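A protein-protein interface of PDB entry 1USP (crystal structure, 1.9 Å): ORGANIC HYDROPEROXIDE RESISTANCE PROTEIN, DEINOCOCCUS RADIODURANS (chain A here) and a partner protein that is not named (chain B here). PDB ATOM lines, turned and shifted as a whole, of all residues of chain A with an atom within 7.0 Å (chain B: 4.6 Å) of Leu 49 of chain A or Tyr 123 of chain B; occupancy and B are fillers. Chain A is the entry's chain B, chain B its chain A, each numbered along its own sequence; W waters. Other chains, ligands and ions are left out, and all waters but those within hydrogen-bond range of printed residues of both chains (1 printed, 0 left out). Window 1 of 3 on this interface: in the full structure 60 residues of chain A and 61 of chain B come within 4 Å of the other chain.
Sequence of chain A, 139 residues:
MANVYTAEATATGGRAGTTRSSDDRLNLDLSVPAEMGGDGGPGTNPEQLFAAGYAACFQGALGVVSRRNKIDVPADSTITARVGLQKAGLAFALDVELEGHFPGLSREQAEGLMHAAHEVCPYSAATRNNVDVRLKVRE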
ATOM      1  N   THR A  19     -15.849  30.743  17.453  1.00  0.00           N
ATOM      2  CA  THR A  19     -17.259  30.531  17.765  1.00  0.00           C
ATOM      3  C   THR A  19     -17.966  31.893  17.803  1.00  0.00           C
ATOM      4  O   THR A  19     -17.473  32.875  18.379  1.00  0.00           O
ATOM      5  CB  THR A  19     -17.424  29.740  19.088  1.00  0.00           C
ATOM      6  OG1 THR A  19     -18.788  29.356  19.264  1.00  0.00           O
ATOM      7  CG2 THR A  19     -17.112  30.603  20.306  1.00  0.00           C
ATOM      8  N   LEU A  26     -21.592  37.614  20.226  1.00  0.00           N
ATOM      9  CA  LEU A  26     -20.384  36.865  20.515  1.00  0.00           C
ATOM     10  C   LEU A  26     -19.688  36.607  19.201  1.00  0.00           C
ATOM     11  O   LEU A  26     -20.292  36.074  18.259  1.00  0.00           O
ATOM     12  CB  LEU A  26     -20.707  35.525  21.157  1.00  0.00           C
ATOM     13  CG  LEU A  26     -21.352  35.530  22.532  1.00  0.00           C
ATOM     14  CD1 LEU A  26     -21.446  34.076  22.997  1.00  0.00           C
ATOM     15  CD2 LEU A  26     -20.563  36.365  23.528  1.00  0.00           C
ATOM     16  N   LEU A  28     -15.864  35.236  18.753  1.00  0.00           N
ATOM     17  CA  LEU A  28     -14.745  34.855  19.602  1.00  0.00           C
ATOM     18  C   LEU A  28     -13.805  33.886  18.899  1.00  0.00           C
ATOM     19  O   LEU A  28     -14.237  33.088  18.066  1.00  0.00           O
ATOM     20  CB  LEU A  28     -15.260  34.210  20.898  1.00  0.00           C
ATOM     21  CG  LEU A  28     -16.082  35.092  21.846  1.00  0.00           C
ATOM     22  CD1 LEU A  28     -16.760  34.248  22.917  1.00  0.00           C
ATOM     23  CD2 LEU A  28     -15.221  36.162  22.493  1.00  0.00           C
ATOM     24  N   ASP A  29     -12.520  33.971  19.232  1.00  0.00           N
ATOM     25  CA  ASP A  29     -11.544  32.969  18.834  1.00  0.00           C
ATOM     26  C   ASP A  29     -11.467  31.883  19.893  1.00  0.00           C
ATOM     27  O   ASP A  29     -11.811  32.102  21.068  1.00  0.00           O
ATOM     28  CB  ASP A  29     -10.160  33.593  18.636  1.00  0.00           C
ATOM     29  CG  ASP A  29     -10.143  34.596  17.504  1.00  0.00           C
ATOM     30  OD1 ASP A  29     -10.646  34.261  16.412  1.00  0.00           O
ATOM     31  OD2 ASP A  29      -9.689  35.753  17.619  1.00  0.00           O
ATOM     32  N   LEU A  30     -10.999  30.722  19.459  1.00  0.00           N
ATOM     33  CA  LEU A  30     -10.846  29.556  20.302  1.00  0.00           C
ATOM     34  C   LEU A  30      -9.378  29.166  20.338  1.00  0.00           C
ATOM     35  O   LEU A  30      -8.723  29.070  19.293  1.00  0.00           O
ATOM     36  CB  LEU A  30     -11.668  28.387  19.754  1.00  0.00           C
ATOM     37  CG  LEU A  30     -13.188  28.550  19.764  1.00  0.00           C
ATOM     38  CD1 LEU A  30     -13.852  27.345  19.093  1.00  0.00           C
ATOM     39  CD2 LEU A  30     -13.704  28.695  21.172  1.00  0.00           C
ATOM     40  N   THR A  44     -10.666  31.756  23.761  1.00  0.00           N
ATOM     41  CA  THR A  44     -11.358  31.119  24.874  1.00  0.00           C
ATOM     42  C   THR A  44     -11.562  29.633  24.589  1.00  0.00           C
ATOM     43  O   THR A  44     -11.013  29.099  23.640  1.00  0.00           O
ATOM     44  CB  THR A  44     -12.710  31.857  25.138  1.00  0.00           C
ATOM     45  OG1 THR A  44     -13.331  31.378  26.335  1.00  0.00           O
ATOM     46  CG2 THR A  44     -13.730  31.569  24.043  1.00  0.00           C
ATOM     47  N   ASN A  45     -12.340  28.956  25.424  1.00  0.00           N
ATOM     48  CA  ASN A  45     -12.526  27.518  25.289  1.00  0.00           C
ATOM     49  C   ASN A  45     -13.885  27.085  25.864  1.00  0.00           C
ATOM     50  O   ASN A  45     -14.510  27.883  26.539  1.00  0.00           O
ATOM     51  CB  ASN A  45     -11.350  26.831  25.998  1.00  0.00           C
ATOM     52  CG  ASN A  45     -11.303  27.150  27.476  1.00  0.00           C
ATOM     53  OD1 ASN A  45     -12.119  26.636  28.247  1.00  0.00           O
ATOM     54  ND2 ASN A  45     -10.351  27.994  27.887  1.00  0.00           N
ATOM     55  N   PRO A  46     -14.356  25.857  25.602  1.00  0.00           N
ATOM     56  CA  PRO A  46     -15.694  25.448  26.068  1.00  0.00           C
ATOM     57  C   PRO A  46     -15.922  25.538  27.586  1.00  0.00           C
ATOM     58  O   PRO A  46     -17.017  25.878  28.012  1.00  0.00           O
ATOM     59  CB  PRO A  46     -15.824  23.987  25.594  1.00  0.00           C
ATOM     60  CG  PRO A  46     -14.759  23.782  24.524  1.00  0.00           C
ATOM     61  CD  PRO A  46     -13.680  24.773  24.862  1.00  0.00           C
ATOM     62  N   GLU A  47     -14.913  25.250  28.394  1.00  0.00           N
ATOM     63  CA  GLU A  47     -15.084  25.270  29.853  1.00  0.00           C
ATOM     64  C   GLU A  47     -15.176  26.703  30.366  1.00  0.00           C
ATOM     65  O   GLU A  47     -15.915  27.005  31.308  1.00  0.00           O
ATOM     66  CB  GLU A  47     -13.948  24.544  30.566  1.00  0.00           C
ATOM     67  CG  GLU A  47     -13.829  23.073  30.201  1.00  0.00           C
ATOM     68  CD  GLU A  47     -13.253  22.821  28.814  1.00  0.00           C
ATOM     69  OE1 GLU A  47     -12.411  23.610  28.350  1.00  0.00           O
ATOM     70  OE2 GLU A  47     -13.660  21.836  28.171  1.00  0.00           O
ATOM     71  N   GLN A  48     -14.440  27.597  29.730  1.00  0.00           N
ATOM     72  CA  GLN A  48     -14.448  28.988  30.146  1.00  0.00           C
ATOM     73  C   GLN A  48     -15.751  29.643  29.719  1.00  0.00           C
ATOM     74  O   GLN A  48     -16.302  30.489  30.442  1.00  0.00           O
ATOM     75  CB  GLN A  48     -13.243  29.704  29.555  1.00  0.00           C
ATOM     76  CG  GLN A  48     -13.016  31.091  30.067  1.00  0.00           C
ATOM     77  CD  GLN A  48     -11.686  31.632  29.562  1.00  0.00           C
ATOM     78  OE1 GLN A  48     -10.695  31.656  30.304  1.00  0.00           O
ATOM     79  NE2 GLN A  48     -11.658  32.037  28.308  1.00  0.00           N
ATOM     80  N   LEU A  49     -16.251  29.251  28.545  1.00  0.00           N
ATOM     81  CA  LEU A  49     -17.552  29.713  28.097  1.00  0.00           C
ATOM     82  C   LEU A  49     -18.659  29.205  29.005  1.00  0.00           C
ATOM     83  O   LEU A  49     -19.614  29.934  29.308  1.00  0.00           O
ATOM     84  CB  LEU A  49     -17.813  29.319  26.633  1.00  0.00           C
ATOM     85  CG  LEU A  49     -17.077  30.205  25.617  1.00  0.00           C
ATOM     86  CD1 LEU A  49     -17.010  29.557  24.250  1.00  0.00           C
ATOM     87  CD2 LEU A  49     -17.754  31.570  25.497  1.00  0.00           C
ATOM     88  N   PHE A  50     -18.527  27.963  29.459  1.00  0.00           N
ATOM     89  CA  PHE A  50     -19.496  27.382  30.380  1.00  0.00           C
ATOM     90  C   PHE A  50     -19.476  28.131  31.707  1.00  0.00           C
ATOM     91  O   PHE A  50     -20.513  28.452  32.256  1.00  0.00           O
ATOM     92  CB  PHE A  50     -19.238  25.892  30.565  1.00  0.00           C
ATOM     93  CG  PHE A  50     -20.326  25.185  31.306  1.00  0.00           C
ATOM     94  CD1 PHE A  50     -21.600  25.040  30.741  1.00  0.00           C
ATOM     95  CD2 PHE A  50     -20.095  24.677  32.566  1.00  0.00           C
ATOM     96  CE1 PHE A  50     -22.613  24.372  31.434  1.00  0.00           C
ATOM     97  CE2 PHE A  50     -21.099  24.017  33.250  1.00  0.00           C
ATOM     98  CZ  PHE A  50     -22.361  23.872  32.686  1.00  0.00           C
ATOM     99  N   ALA A  51     -18.286  28.437  32.209  1.00  0.00           N
ATOM    100  CA  ALA A  51     -18.158  29.206  33.432  1.00  0.00           C
ATOM    101  C   ALA A  51     -18.798  30.608  33.318  1.00  0.00           C
ATOM    102  O   ALA A  51     -19.500  31.050  34.238  1.00  0.00           O
ATOM    103  CB  ALA A  51     -16.703  29.317  33.809  1.00  0.00           C
ATOM    104  N   ALA A  52     -18.560  31.309  32.209  1.00  0.00           N
ATOM    105  CA  ALA A  52     -19.090  32.670  32.046  1.00  0.00           C
ATOM    106  C   ALA A  52     -20.612  32.635  31.935  1.00  0.00           C
ATOM    107  O   ALA A  52     -21.301  33.513  32.444  1.00  0.00           O
ATOM    108  CB  ALA A  52     -18.488  33.342  30.826  1.00  0.00           C
ATOM    109  N   GLY A  53     -21.114  31.588  31.276  1.00  0.00           N
ATOM    110  CA  GLY A  53     -22.527  31.428  31.057  1.00  0.00           C
ATOM    111  C   GLY A  53     -23.258  31.071  32.327  1.00  0.00           C
ATOM    112  O   GLY A  53     -24.356  31.553  32.550  1.00  0.00           O
ATOM    113  N   TYR A  54     -22.665  30.198  33.137  1.00  0.00           N
ATOM    114  CA  TYR A  54     -23.303  29.714  34.364  1.00  0.00           C
ATOM    115  C   TYR A  54     -23.355  30.848  35.380  1.00  0.00           C
ATOM    116  O   TYR A  54     -24.369  31.057  36.024  1.00  0.00           O
ATOM    117  CB  TYR A  54     -22.546  28.507  34.938  1.00  0.00           C
ATOM    118  CG  TYR A  54     -23.390  27.491  35.672  1.00  0.00           C
ATOM    119  CD1 TYR A  54     -23.018  26.153  35.717  1.00  0.00           C
ATOM    120  CD2 TYR A  54     -24.535  27.862  36.367  1.00  0.00           C
ATOM    121  CE1 TYR A  54     -23.787  25.215  36.404  1.00  0.00           C
ATOM    122  CE2 TYR A  54     -25.294  26.933  37.051  1.00  0.00           C
ATOM    123  CZ  TYR A  54     -24.926  25.629  37.072  1.00  0.00           C
ATOM    124  OH  TYR A  54     -25.694  24.730  37.762  1.00  0.00           O
ATOM    125  N   ALA A  55     -22.267  31.597  35.489  1.00  0.00           N
ATOM    126  CA  ALA A  55     -22.208  32.754  36.373  1.00  0.00           C
ATOM    127  C   ALA A  55     -23.278  33.761  35.974  1.00  0.00           C
ATOM    128  O   ALA A  55     -24.008  34.280  36.826  1.00  0.00           O
ATOM    129  CB  ALA A  55     -20.845  33.403  36.300  1.00  0.00           C
ATOM    130  N   VAL A  83     -15.124  26.022  36.779  1.00  0.00           N
ATOM    131  CA  VAL A  83     -15.482  24.848  36.003  1.00  0.00           C
ATOM    132  C   VAL A  83     -14.233  24.026  35.671  1.00  0.00           C
ATOM    133  O   VAL A  83     -13.373  24.486  34.920  1.00  0.00           O
ATOM    134  CB  VAL A  83     -16.165  25.243  34.677  1.00  0.00           C
ATOM    135  CG1 VAL A  83     -16.461  23.997  33.831  1.00  0.00           C
ATOM    136  CG2 VAL A  83     -17.451  26.036  34.934  1.00  0.00           C
ATOM    137  N   PHE A  92     -14.445  12.529  29.317  1.00  0.00           N
ATOM    138  CA  PHE A  92     -14.551  13.928  29.767  1.00  0.00           C
ATOM    139  C   PHE A  92     -15.844  14.263  30.547  1.00  0.00           C
ATOM    140  O   PHE A  92     -16.953  13.922  30.123  1.00  0.00           O
ATOM    141  CB  PHE A  92     -14.406  14.887  28.584  1.00  0.00           C
ATOM    142  CG  PHE A  92     -13.079  14.788  27.889  1.00  0.00           C
ATOM    143  CD1 PHE A  92     -12.958  14.082  26.697  1.00  0.00           C
ATOM    144  CD2 PHE A  92     -11.943  15.373  28.442  1.00  0.00           C
ATOM    145  CE1 PHE A  92     -11.723  13.973  26.057  1.00  0.00           C
ATOM    146  CE2 PHE A  92     -10.710  15.276  27.813  1.00  0.00           C
ATOM    147  CZ  PHE A  92     -10.596  14.576  26.615  1.00  0.00           C
ATOM    148  N   ALA A  93     -15.676  14.940  31.689  1.00  0.00           N
ATOM    149  CA  ALA A  93     -16.788  15.457  32.483  1.00  0.00           C
ATOM    150  C   ALA A  93     -16.456  16.823  33.084  1.00  0.00           C
ATOM    151  O   ALA A  93     -15.283  17.164  33.288  1.00  0.00           O
ATOM    152  CB  ALA A  93     -17.139  14.497  33.577  1.00  0.00           C
ATOM    153  N   LEU A  94     -17.499  17.589  33.393  1.00  0.00           N
ATOM    154  CA  LEU A  94     -17.338  18.904  33.980  1.00  0.00           C
ATOM    155  C   LEU A  94     -17.640  18.818  35.461  1.00  0.00           C
ATOM    156  O   LEU A  94     -18.433  18.002  35.897  1.00  0.00           O
ATOM    157  CB  LEU A  94     -18.265  19.914  33.323  1.00  0.00           C
ATOM    158  CG  LEU A  94     -18.048  20.157  31.832  1.00  0.00           C
ATOM    159  CD1 LEU A  94     -19.209  20.944  31.256  1.00  0.00           C
ATOM    160  CD2 LEU A  94     -16.725  20.900  31.585  1.00  0.00           C
ATOM    161  N   TYR A 123     -29.284  26.351  33.515  1.00  0.00           N
ATOM    162  CA  TYR A 123     -28.036  25.552  33.469  1.00  0.00           C
ATOM    163  C   TYR A 123     -28.064  24.475  34.566  1.00  0.00           C
ATOM    164  O   TYR A 123     -27.624  23.357  34.345  1.00  0.00           O
ATOM    165  CB  TYR A 123     -26.807  26.403  33.710  1.00  0.00           C
ATOM    166  CG  TYR A 123     -26.220  27.150  32.533  1.00  0.00           C
ATOM    167  CD1 TYR A 123     -27.014  27.940  31.700  1.00  0.00           C
ATOM    168  CD2 TYR A 123     -24.844  27.100  32.278  1.00  0.00           C
ATOM    169  CE1 TYR A 123     -26.459  28.658  30.660  1.00  0.00           C
ATOM    170  CE2 TYR A 123     -24.282  27.817  31.246  1.00  0.00           C
ATOM    171  CZ  TYR A 123     -25.096  28.599  30.435  1.00  0.00           C
ATOM    172  OH  TYR A 123     -24.530  29.319  29.406  1.00  0.00           O
ATOM    173  N   ALA A 126     -30.454  21.804  33.469  1.00  0.00           N
ATOM    174  CA  ALA A 126     -29.788  21.084  32.371  1.00  0.00           C
ATOM    175  C   ALA A 126     -28.729  20.098  32.811  1.00  0.00           C
ATOM    176  O   ALA A 126     -28.562  19.066  32.178  1.00  0.00           O
ATOM    177  CB  ALA A 126     -29.178  22.064  31.386  1.00  0.00           C
ATOM    178  N   THR A 127     -28.036  20.391  33.905  1.00  0.00           N
ATOM    179  CA  THR A 127     -26.901  19.584  34.312  1.00  0.00           C
ATOM    180  C   THR A 127     -27.196  18.754  35.551  1.00  0.00           C
ATOM    181  O   THR A 127     -26.301  18.084  36.049  1.00  0.00           O
ATOM    182  CB  THR A 127     -25.648  20.450  34.514  1.00  0.00           C
ATOM    183  OG1 THR A 127     -25.859  21.411  35.557  1.00  0.00           O
ATOM    184  CG2 THR A 127     -25.349  21.303  33.265  1.00  0.00           C
ATOM    185  N   LEU B  26     -12.257  36.356  28.241  1.00  0.00           N
ATOM    186  CA  LEU B  26     -13.655  36.745  28.071  1.00  0.00           C
ATOM    187  C   LEU B  26     -13.942  38.009  28.864  1.00  0.00           C
ATOM    188  O   LEU B  26     -13.690  38.056  30.048  1.00  0.00           O
ATOM    189  CB  LEU B  26     -14.585  35.636  28.547  1.00  0.00           C
ATOM    190  CG  LEU B  26     -14.678  34.396  27.675  1.00  0.00           C
ATOM    191  CD1 LEU B  26     -15.715  33.423  28.241  1.00  0.00           C
ATOM    192  CD2 LEU B  26     -14.989  34.750  26.239  1.00  0.00           C
ATOM    193  N   LEU B  49     -24.359  32.097  25.353  1.00  0.00           N
ATOM    194  CA  LEU B  49     -23.049  31.624  25.803  1.00  0.00           C
ATOM    195  C   LEU B  49     -23.025  30.089  25.758  1.00  0.00           C
ATOM    196  O   LEU B  49     -22.043  29.481  25.331  1.00  0.00           O
ATOM    197  CB  LEU B  49     -22.713  32.164  27.196  1.00  0.00           C
ATOM    198  CG  LEU B  49     -22.207  33.618  27.187  1.00  0.00           C
ATOM    199  CD1 LEU B  49     -22.360  34.287  28.551  1.00  0.00           C
ATOM    200  CD2 LEU B  49     -20.752  33.654  26.738  1.00  0.00           C
ATOM    201  N   PHE B  50     -24.138  29.469  26.122  1.00  0.00           N
ATOM    202  CA  PHE B  50     -24.231  28.007  26.083  1.00  0.00           C
ATOM    203  C   PHE B  50     -24.095  27.496  24.644  1.00  0.00           C
ATOM    204  O   PHE B  50     -23.415  26.500  24.398  1.00  0.00           O
ATOM    205  CB  PHE B  50     -25.545  27.532  26.739  1.00  0.00           C
ATOM    206  CG  PHE B  50     -25.539  26.067  27.103  1.00  0.00           C
ATOM    207  CD1 PHE B  50     -24.795  25.609  28.170  1.00  0.00           C
ATOM    208  CD2 PHE B  50     -26.234  25.150  26.334  1.00  0.00           C
ATOM    209  CE1 PHE B  50     -24.787  24.243  28.491  1.00  0.00           C
ATOM    210  CE2 PHE B  50     -26.238  23.795  26.639  1.00  0.00           C
ATOM    211  CZ  PHE B  50     -25.508  23.334  27.704  1.00  0.00           C
ATOM    212  N   ALA B  52     -22.630  29.032  22.097  1.00  0.00           N
ATOM    213  CA  ALA B  52     -21.265  29.238  21.639  1.00  0.00           C
ATOM    214  C   ALA B  52     -20.325  28.194  22.215  1.00  0.00           C
ATOM    215  O   ALA B  52     -19.451  27.683  21.512  1.00  0.00           O
ATOM    216  CB  ALA B  52     -20.799  30.627  21.984  1.00  0.00           C
ATOM    217  N   GLY B  53     -20.516  27.861  23.486  1.00  0.00           N
ATOM    218  CA  GLY B  53     -19.673  26.880  24.151  1.00  0.00           C
ATOM    219  C   GLY B  53     -19.909  25.458  23.676  1.00  0.00           C
ATOM    220  O   GLY B  53     -18.966  24.692  23.481  1.00  0.00           O
ATOM    221  N   TYR B  54     -21.167  25.100  23.461  1.00  0.00           N
ATOM    222  CA  TYR B  54     -21.518  23.733  23.041  1.00  0.00           C
ATOM    223  C   TYR B  54     -21.019  23.483  21.617  1.00  0.00           C
ATOM    224  O   TYR B  54     -20.513  22.409  21.314  1.00  0.00           O
ATOM    225  CB  TYR B  54     -23.038  23.527  23.087  1.00  0.00           C
ATOM    226  CG  TYR B  54     -23.533  22.132  23.382  1.00  0.00           C
ATOM    227  CD1 TYR B  54     -22.796  21.000  23.054  1.00  0.00           C
ATOM    228  CD2 TYR B  54     -24.777  21.952  23.988  1.00  0.00           C
ATOM    229  CE1 TYR B  54     -23.291  19.704  23.322  1.00  0.00           C
ATOM    230  CE2 TYR B  54     -25.266  20.672  24.276  1.00  0.00           C
ATOM    231  CZ  TYR B  54     -24.518  19.556  23.931  1.00  0.00           C
ATOM    232  OH  TYR B  54     -25.003  18.304  24.204  1.00  0.00           O
ATOM    233  N   CYS B  57     -17.318  22.960  21.886  1.00  0.00           N
ATOM    234  CA  CYS B  57     -17.031  21.682  22.543  1.00  0.00           C
ATOM    235  C   CYS B  57     -17.156  20.533  21.550  1.00  0.00           C
ATOM    236  O   CYS B  57     -16.371  19.589  21.565  1.00  0.00           O
ATOM    237  CB  CYS B  57     -18.021  21.477  23.699  1.00  0.00           C
ATOM    238  SG  CYS B  57     -17.694  20.023  24.730  1.00  0.00           S
ATOM    239  N   CYS B 121     -18.167  14.729  23.892  1.00  0.00           N
ATOM    240  CA  CYS B 121     -18.320  16.116  24.308  1.00  0.00           C
ATOM    241  C   CYS B 121     -18.770  16.213  25.765  1.00  0.00           C
ATOM    242  O   CYS B 121     -19.793  15.643  26.102  1.00  0.00           O
ATOM    243  CB  CYS B 121     -19.359  16.776  23.390  1.00  0.00           C
ATOM    244  SG  CYS B 121     -19.864  18.411  23.893  1.00  0.00           S
ATOM    245  N   PRO B 122     -18.025  16.902  26.638  1.00  0.00           N
ATOM    246  CA  PRO B 122     -18.464  17.072  28.028  1.00  0.00           C
ATOM    247  C   PRO B 122     -19.774  17.841  28.233  1.00  0.00           C
ATOM    248  O   PRO B 122     -20.426  17.585  29.232  1.00  0.00           O
ATOM    249  CB  PRO B 122     -17.277  17.786  28.692  1.00  0.00           C
ATOM    250  CG  PRO B 122     -16.534  18.388  27.610  1.00  0.00           C
ATOM    251  CD  PRO B 122     -16.680  17.470  26.431  1.00  0.00           C
ATOM    252  N   TYR B 123     -20.151  18.742  27.325  1.00  0.00           N
ATOM    253  CA  TYR B 123     -21.447  19.421  27.439  1.00  0.00           C
ATOM    254  C   TYR B 123     -22.558  18.378  27.260  1.00  0.00           C
ATOM    255  O   TYR B 123     -23.580  18.427  27.944  1.00  0.00           O
ATOM    256  CB  TYR B 123     -21.618  20.526  26.385  1.00  0.00           C
ATOM    257  CG  TYR B 123     -21.044  21.910  26.675  1.00  0.00           C
ATOM    258  CD1 TYR B 123     -19.714  22.084  27.041  1.00  0.00           C
ATOM    259  CD2 TYR B 123     -21.823  23.057  26.493  1.00  0.00           C
ATOM    260  CE1 TYR B 123     -19.194  23.345  27.258  1.00  0.00           C
ATOM    261  CE2 TYR B 123     -21.293  24.324  26.690  1.00  0.00           C
ATOM    262  CZ  TYR B 123     -19.986  24.456  27.076  1.00  0.00           C
ATOM    263  OH  TYR B 123     -19.454  25.713  27.278  1.00  0.00           O
ATOM    264  N   SER B 124     -22.365  17.438  26.326  1.00  0.00           N
ATOM    265  CA  SER B 124     -23.310  16.336  26.130  1.00  0.00           C
ATOM    266  C   SER B 124     -23.399  15.415  27.346  1.00  0.00           C
ATOM    267  O   SER B 124     -24.508  15.003  27.752  1.00  0.00           O
ATOM    268  CB  SER B 124     -22.969  15.517  24.873  1.00  0.00           C
ATOM    269  OG  SER B 124     -23.089  16.292  23.688  1.00  0.00           O
ATOM    270  N   ALA B 125     -22.253  15.097  27.935  1.00  0.00           N
ATOM    271  CA  ALA B 125     -22.236  14.321  29.179  1.00  0.00           C
ATOM    272  C   ALA B 125     -22.981  15.056  30.291  1.00  0.00           C
ATOM    273  O   ALA B 125     -23.761  14.461  31.030  1.00  0.00           O
ATOM    274  CB  ALA B 125     -20.806  14.029  29.603  1.00  0.00           C
ATOM    275  N   ALA B 126     -22.755  16.364  30.387  1.00  0.00           N
ATOM    276  CA  ALA B 126     -23.372  17.204  31.423  1.00  0.00           C
ATOM    277  C   ALA B 126     -24.878  17.274  31.328  1.00  0.00           C
ATOM    278  O   ALA B 126     -25.543  17.395  32.354  1.00  0.00           O
ATOM    279  CB  ALA B 126     -22.807  18.627  31.350  1.00  0.00           C
ATOM    280  N   THR B 127     -25.410  17.232  30.101  1.00  0.00           N
ATOM    281  CA  THR B 127     -26.834  17.458  29.878  1.00  0.00           C
ATOM    282  C   THR B 127     -27.605  16.185  29.565  1.00  0.00           C
ATOM    283  O   THR B 127     -28.818  16.230  29.330  1.00  0.00           O
ATOM    284  CB  THR B 127     -27.056  18.454  28.733  1.00  0.00           C
ATOM    285  OG1 THR B 127     -26.435  17.982  27.532  1.00  0.00           O
ATOM    286  CG2 THR B 127     -26.399  19.786  29.055  1.00  0.00           C
HETATM  287  O   HOH W   1     -19.743  16.885  31.855  1.00  0.00           O
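Printed residues of chain B within 4 Å of Pro 46 of chain A: Gly 53 (3.9 Å), Cys 57 (3.7 Å) and Tyr 123 (2.6 Å). Of chain B, only Leu 26 (3.9 Å), Leu 49 (3.9 Å), Gly 53 (3.8 Å) and Tyr 123 (3.98 Å) come within 4 Å of Leu 49 of chain A. Of the printed residues of chain B, Ala 52 of chain A touches Leu 26. Ala 55 of chain A touches none of the printed residues of chain B. Of the printed residues of chain B, Ala 126 of chain A touches Ala 126 (3.5 Å) and Thr 127 (3.3 Å). Of the printed residues of chain A, Phe 50 of chain B touches Phe 50 and Tyr 123. Tyr 123 of chain B touches just these residues of chain A: Pro 46, Leu 49 and Phe 50. The nearest printed residue of chain B that does not touch Ala 126 of chain A is Phe 50 of chain B (5.4 Å).
The side-chain sulfur (SG) of Cys 57 of chain B sits close to the backbone NH (N) of Tyr 123 of chain B (3.8 Å). The side-chain sulfur of Cys 121 of chain B sits close to the backbone NH of Tyr 123 of chain B. O of Tyr 123 of chain B sits at hydrogen-bond distance from OG1 of Thr 127 of chain B. O of Thr 19 of chain A is in hydrogen-bond range of N of Leu 28 of chain A. OG1 of Thr 44 of chain A lies within hydrogen-bond range of NE2 of Gln 48 of chain A. The backbone carbonyl oxygen (O) of Tyr 123 of chain A lies within hydrogen-bond range of the side-chain hydroxyl (OG1) of Thr 127 of chain A.
Water W1 lies within hydrogen-bond range of the backbone carbonyl oxygen of Pro 122 of chain B, the backbone NH of Leu 94 of chain A and the backbone NH of Ala 126 of chain B.
Hydrophobic or aromatic side chains of chain A within 4 Å of the printed part of chain B: Leu 26, Leu 28, Pro 46, Leu 49, Phe 50, Ala 52 and Tyr 123. Of the 14 printed residues of chain B, 10 touch a printed residue of chain A. Hydrophobic or aromatic side chains of chain B within 4 Å of the printed part of chain A: Leu 26, Leu 49, Phe 50, Ala 52, Tyr 123 and Ala 125. Along chain B the printed residues that touch a printed residue of chain A span positions 26 to 127. Among the printed residues, 22 pairs touch across the chains. Among the printed residues, no Asp or Glu carboxylate lies within 4 Å of a Lys or Arg side-chain nitrogen of the other chain.
Leu 26 of chain A touches Ala 52 of chain B. Gly 53 of chain B touches Pro 46 of chain A. Pro 46 of chain A touches Cys 57 of chain B. Leu 26 of chain B touches Gln 48 of chain A. Leu 49 of chain A touches Leu 26 of chain B. CD2 of Leu 49 of chain A touches CD2 of Leu 49 of chain B (3.9 Å). Phe 50 of chain B touches Phe 50 of chain A. Leu 26 of chain B touches Ala 52 of chain A (CD1 to CB, 3.8 Å). Leu 49 of chain B touches Gly 53 of chain A (CD1 to CA, 3.8 Å). Ala 126 of chain B touches Thr 127 of chain A.
OH of Tyr 123 of chain A sits at hydrogen-bond distance from N of Phe 50 of chain B (3.3 Å). O of Ala 52 of chain B sits at hydrogen-bond distance from OG1 of Thr 19 of chain A, at 2.9 Å. The side-chain hydroxyl (OH) of Tyr 123 of chain B is in hydrogen-bond range of the backbone carbonyl oxygen (O) of Pro 46 of chain A. OH of Tyr 123 of chain B lies within hydrogen-bond range of N of Phe 50 of chain A (3.3 Å). The backbone carbonyl oxygen (O) of Ala 126 of chain B sits close to the backbone carbonyl oxygen (O) of Ala 126 of chain A (3.5 Å).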
